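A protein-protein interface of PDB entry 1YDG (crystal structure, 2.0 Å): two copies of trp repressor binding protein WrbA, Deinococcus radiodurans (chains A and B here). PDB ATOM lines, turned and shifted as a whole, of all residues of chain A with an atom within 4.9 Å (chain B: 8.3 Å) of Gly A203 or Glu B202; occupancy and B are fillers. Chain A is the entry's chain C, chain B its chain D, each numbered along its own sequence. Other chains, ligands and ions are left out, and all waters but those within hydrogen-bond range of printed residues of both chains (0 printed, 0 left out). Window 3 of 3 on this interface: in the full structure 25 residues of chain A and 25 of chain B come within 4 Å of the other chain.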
ATOM      1  N   LYS A 199       0.101  13.920  29.376  1.00  0.00           N
ATOM      2  CA  LYS A 199      -0.122  14.650  28.112  1.00  0.00           C
ATOM      3  C   LYS A 199       0.866  14.223  27.046  1.00  0.00           C
ATOM      4  O   LYS A 199       0.504  14.056  25.875  1.00  0.00           O
ATOM      5  CB  LYS A 199      -0.047  16.165  28.310  1.00  0.00           C
ATOM      6  CG  LYS A 199      -1.251  16.702  29.050  1.00  0.00           C
ATOM      7  CD  LYS A 199      -1.180  18.198  29.316  1.00  0.00           C
ATOM      8  CE  LYS A 199      -2.117  18.571  30.458  1.00  0.00           C
ATOM      9  NZ  LYS A 199      -2.628  19.982  30.371  1.00  0.00           N
ATOM     10  N   LEU A 200       2.113  14.051  27.465  1.00  0.00           N
ATOM     11  CA  LEU A 200       3.183  13.590  26.584  1.00  0.00           C
ATOM     12  C   LEU A 200       2.838  12.240  25.941  1.00  0.00           C
ATOM     13  O   LEU A 200       3.048  12.031  24.756  1.00  0.00           O
ATOM     14  CB  LEU A 200       4.475  13.425  27.386  1.00  0.00           C
ATOM     15  CG  LEU A 200       5.819  13.965  26.876  1.00  0.00           C
ATOM     16  CD1 LEU A 200       6.934  12.949  27.249  1.00  0.00           C
ATOM     17  CD2 LEU A 200       5.883  14.288  25.376  1.00  0.00           C
ATOM     18  N   LEU A 201       2.337  11.328  26.760  1.00  0.00           N
ATOM     19  CA  LEU A 201       2.072   9.958  26.337  1.00  0.00           C
ATOM     20  C   LEU A 201       0.832   9.883  25.483  1.00  0.00           C
ATOM     21  O   LEU A 201       0.779   9.105  24.535  1.00  0.00           O
ATOM     22  CB  LEU A 201       1.878   9.062  27.555  1.00  0.00           C
ATOM     23  CG  LEU A 201       3.098   8.856  28.438  1.00  0.00           C
ATOM     24  CD1 LEU A 201       2.666   8.214  29.726  1.00  0.00           C
ATOM     25  CD2 LEU A 201       4.133   8.017  27.741  1.00  0.00           C
ATOM     26  N   GLU A 202      -0.161  10.682  25.855  1.00  0.00           N
ATOM     27  CA  GLU A 202      -1.407  10.823  25.106  1.00  0.00           C
ATOM     28  C   GLU A 202      -1.167  11.315  23.664  1.00  0.00           C
ATOM     29  O   GLU A 202      -1.707  10.747  22.725  1.00  0.00           O
ATOM     30  CB  GLU A 202      -2.334  11.798  25.841  1.00  0.00           C
ATOM     31  CG  GLU A 202      -3.723  11.283  26.076  1.00  0.00           C
ATOM     32  CD  GLU A 202      -4.571  11.336  24.824  1.00  0.00           C
ATOM     33  OE1 GLU A 202      -5.053  10.265  24.390  1.00  0.00           O
ATOM     34  OE2 GLU A 202      -4.736  12.451  24.279  1.00  0.00           O
ATOM     35  N   GLY A 203      -0.354  12.360  23.499  1.00  0.00           N
ATOM     36  CA  GLY A 203      -0.024  12.890  22.172  1.00  0.00           C
ATOM     37  C   GLY A 203       0.924  12.060  21.322  1.00  0.00           C
ATOM     38  O   GLY A 203       1.017  12.259  20.100  1.00  0.00           O
ATOM     39  N   GLY A 204       1.638  11.132  21.950  1.00  0.00           N
ATOM     40  CA  GLY A 204       2.516  10.214  21.222  1.00  0.00           C
ATOM     41  C   GLY A 204       1.838   8.907  20.828  1.00  0.00           C
ATOM     42  O   GLY A 204       2.515   7.980  20.370  1.00  0.00           O
ATOM     43  N   SER A 205       0.510   8.865  20.980  1.00  0.00           N
ATOM     44  CA  SER A 205      -0.339   7.661  20.861  1.00  0.00           C
ATOM     45  C   SER A 205      -1.080   7.480  22.181  1.00  0.00           C
ATOM     46  O   SER A 205      -2.252   7.846  22.331  1.00  0.00           O
ATOM     47  CB  SER A 205       0.444   6.375  20.530  1.00  0.00           C
ATOM     48  OG  SER A 205      -0.370   5.223  20.719  1.00  0.00           O
ATOM     49  N   THR B   4      -4.322  20.868  15.107  1.00  0.00           N
ATOM     50  CA  THR B   4      -4.057  21.116  13.656  1.00  0.00           C
ATOM     51  C   THR B   4      -2.936  22.155  13.488  1.00  0.00           C
ATOM     52  O   THR B   4      -2.079  21.992  12.626  1.00  0.00           O
ATOM     53  CB  THR B   4      -5.375  21.508  12.860  1.00  0.00           C
ATOM     54  OG1 THR B   4      -5.375  20.908  11.552  1.00  0.00           O
ATOM     55  CG2 THR B   4      -5.546  23.024  12.707  1.00  0.00           C
ATOM     56  N   VAL B   7       3.268  23.839  15.609  1.00  0.00           N
ATOM     57  CA  VAL B   7       3.993  24.226  16.826  1.00  0.00           C
ATOM     58  C   VAL B   7       4.573  25.620  16.647  1.00  0.00           C
ATOM     59  O   VAL B   7       5.255  25.893  15.665  1.00  0.00           O
ATOM     60  CB  VAL B   7       5.136  23.228  17.142  1.00  0.00           C
ATOM     61  CG1 VAL B   7       6.048  23.760  18.255  1.00  0.00           C
ATOM     62  CG2 VAL B   7       4.570  21.856  17.526  1.00  0.00           C
ATOM     63  N   GLU B 195       9.015  17.926  18.015  1.00  0.00           N
ATOM     64  CA  GLU B 195       8.263  16.669  18.139  1.00  0.00           C
ATOM     65  C   GLU B 195       7.669  16.480  19.533  1.00  0.00           C
ATOM     66  O   GLU B 195       6.505  16.109  19.666  1.00  0.00           O
ATOM     67  CB  GLU B 195       9.160  15.478  17.757  1.00  0.00           C
ATOM     68  CG  GLU B 195       9.504  15.475  16.254  1.00  0.00           C
ATOM     69  CD  GLU B 195      10.495  14.408  15.851  1.00  0.00           C
ATOM     70  OE1 GLU B 195      11.076  13.730  16.749  1.00  0.00           O
ATOM     71  OE2 GLU B 195      10.706  14.255  14.630  1.00  0.00           O
ATOM     72  N   LEU B 196       8.468  16.741  20.565  1.00  0.00           N
ATOM     73  CA  LEU B 196       8.005  16.665  21.951  1.00  0.00           C
ATOM     74  C   LEU B 196       6.918  17.687  22.248  1.00  0.00           C
ATOM     75  O   LEU B 196       5.936  17.366  22.922  1.00  0.00           O
ATOM     76  CB  LEU B 196       9.164  16.864  22.933  1.00  0.00           C
ATOM     77  CG  LEU B 196      10.133  15.688  23.129  1.00  0.00           C
ATOM     78  CD1 LEU B 196      11.426  16.174  23.751  1.00  0.00           C
ATOM     79  CD2 LEU B 196       9.529  14.565  23.957  1.00  0.00           C
ATOM     80  N   THR B 197       7.097  18.915  21.757  1.00  0.00           N
ATOM     81  CA  THR B 197       6.123  19.979  21.986  1.00  0.00           C
ATOM     82  C   THR B 197       4.786  19.636  21.344  1.00  0.00           C
ATOM     83  O   THR B 197       3.740  19.812  21.949  1.00  0.00           O
ATOM     84  CB  THR B 197       6.620  21.347  21.429  1.00  0.00           C
ATOM     85  OG1 THR B 197       7.978  21.558  21.797  1.00  0.00           O
ATOM     86  CG2 THR B 197       5.776  22.480  21.956  1.00  0.00           C
ATOM     87  N   ALA B 198       4.821  19.139  20.111  1.00  0.00           N
ATOM     88  CA  ALA B 198       3.588  18.724  19.435  1.00  0.00           C
ATOM     89  C   ALA B 198       2.825  17.680  20.263  1.00  0.00           C
ATOM     90  O   ALA B 198       1.602  17.726  20.397  1.00  0.00           O
ATOM     91  CB  ALA B 198       3.924  18.190  18.044  1.00  0.00           C
ATOM     92  N   LYS B 199       3.568  16.757  20.852  1.00  0.00           N
ATOM     93  CA  LYS B 199       2.999  15.693  21.662  1.00  0.00           C
ATOM     94  C   LYS B 199       2.347  16.202  22.942  1.00  0.00           C
ATOM     95  O   LYS B 199       1.223  15.830  23.269  1.00  0.00           O
ATOM     96  CB  LYS B 199       4.076  14.667  21.987  1.00  0.00           C
ATOM     97  CG  LYS B 199       4.309  13.686  20.856  1.00  0.00           C
ATOM     98  CD  LYS B 199       5.532  12.813  21.129  1.00  0.00           C
ATOM     99  CE  LYS B 199       5.596  11.627  20.184  1.00  0.00           C
ATOM    100  NZ  LYS B 199       6.994  11.178  19.932  1.00  0.00           N
ATOM    101  N   LEU B 200       3.057  17.046  23.675  1.00  0.00           N
ATOM    102  CA  LEU B 200       2.494  17.679  24.867  1.00  0.00           C
ATOM    103  C   LEU B 200       1.214  18.459  24.560  1.00  0.00           C
ATOM    104  O   LEU B 200       0.238  18.388  25.315  1.00  0.00           O
ATOM    105  CB  LEU B 200       3.524  18.624  25.504  1.00  0.00           C
ATOM    106  CG  LEU B 200       4.447  17.875  26.462  1.00  0.00           C
ATOM    107  CD1 LEU B 200       5.819  18.545  26.598  1.00  0.00           C
ATOM    108  CD2 LEU B 200       3.755  17.710  27.837  1.00  0.00           C
ATOM    109  N   LEU B 201       1.226  19.201  23.461  1.00  0.00           N
ATOM    110  CA  LEU B 201       0.094  20.047  23.102  1.00  0.00           C
ATOM    111  C   LEU B 201      -1.109  19.231  22.665  1.00  0.00           C
ATOM    112  O   LEU B 201      -2.242  19.594  22.971  1.00  0.00           O
ATOM    113  CB  LEU B 201       0.477  20.991  21.972  1.00  0.00           C
ATOM    114  CG  LEU B 201       1.501  22.071  22.268  1.00  0.00           C
ATOM    115  CD1 LEU B 201       1.830  22.739  20.948  1.00  0.00           C
ATOM    116  CD2 LEU B 201       0.965  23.072  23.288  1.00  0.00           C
ATOM    117  N   GLU B 202      -0.851  18.149  21.932  1.00  0.00           N
ATOM    118  CA  GLU B 202      -1.903  17.201  21.550  1.00  0.00           C
ATOM    119  C   GLU B 202      -2.507  16.519  22.781  1.00  0.00           C
ATOM    120  O   GLU B 202      -3.721  16.388  22.869  1.00  0.00           O
ATOM    121  CB  GLU B 202      -1.375  16.158  20.563  1.00  0.00           C
ATOM    122  CG  GLU B 202      -2.283  14.932  20.375  1.00  0.00           C
ATOM    123  CD  GLU B 202      -3.666  15.263  19.825  1.00  0.00           C
ATOM    124  OE1 GLU B 202      -4.673  14.816  20.433  1.00  0.00           O
ATOM    125  OE2 GLU B 202      -3.755  15.965  18.791  1.00  0.00           O
ATOM    126  N   GLY B 203      -1.668  16.092  23.726  1.00  0.00           N
ATOM    127  CA  GLY B 203      -2.161  15.447  24.949  1.00  0.00           C
ATOM    128  C   GLY B 203      -3.091  16.298  25.803  1.00  0.00           C
ATOM    129  O   GLY B 203      -4.033  15.781  26.409  1.00  0.00           O
ATOM    130  N   GLY B 204      -2.826  17.604  25.846  1.00  0.00           N
ATOM    131  CA  GLY B 204      -3.694  18.566  26.535  1.00  0.00           C
ATOM    132  C   GLY B 204      -4.848  19.122  25.704  1.00  0.00           C
ATOM    133  O   GLY B 204      -5.773  19.724  26.250  1.00  0.00           O
ATOM    134  N   SER B 205      -4.787  18.948  24.383  1.00  0.00           N
ATOM    135  CA  SER B 205      -5.880  19.356  23.483  1.00  0.00           C
ATOM    136  C   SER B 205      -5.921  18.448  22.256  1.00  0.00           C
ATOM    137  O   SER B 205      -6.624  17.429  22.252  1.00  0.00           O
ATOM    138  CB  SER B 205      -5.720  20.825  23.055  1.00  0.00           C
ATOM    139  OG  SER B 205      -6.823  21.275  22.272  1.00  0.00           O
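Lys A199 touches Leu B200, and with the chains exchanged Leu A200 touches Lys B199. Lys A199 touches Gly B203, and with the chains exchanged Gly A203 touches Lys B199. Glu A202 touches Gly B203, and with the chains exchanged Gly A203 touches Glu B202. Gly A203 touches its own counterpart, Gly B203. 7 positions are printed for both chains.
Along chain A the printed residues that touch a printed residue of chain B span positions 199 to 204. Hydrophobic or aromatic side chains of chain B that line the printed part of chain A: Leu B196. Among the printed residues, no Asp or Glu carboxylate lies within 4 Å of a Lys or Arg side-chain nitrogen of the other chain.
The backbone carbonyl oxygen of Lys A199 lies close to the backbone carbonyl oxygen of Lys B199, at 3.2 Å.
Gly A203 touches three residues of chain B. Of the printed residues of chain B, Gly A204 touches Lys B199 (3.5 Å). Glu B202 touches just one residue of chain A: Gly A203. Of the printed residues of chain A, Gly B203 touches Lys A199 (3.1 Å), Glu A202 (3.8 Å) and Gly A203 (3.9 Å). The nearest printed residue of chain B that does not touch Gly A203 is Leu B200 (5.4 Å).
Among the printed residues, pairs that only touch across the chains: Lys A199 with Gly B203 (3.1 Å), Gly A203 with Lys B199 (3.4 Å), Gly A203 with Glu B202 (3.5 Å), Gly A204 with Lys B199 (3.5 Å), Lys A199 with Gly B204 (3.7 Å), Lys A199 with Leu B200 (3.7 Å), Glu A202 with Gly B203 (3.8 Å), Leu A200 with Lys B199 (3.9 Å), Gly A203 with Gly B203 (3.9 Å) and Leu A200 with Leu B196 (3.9 Å).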
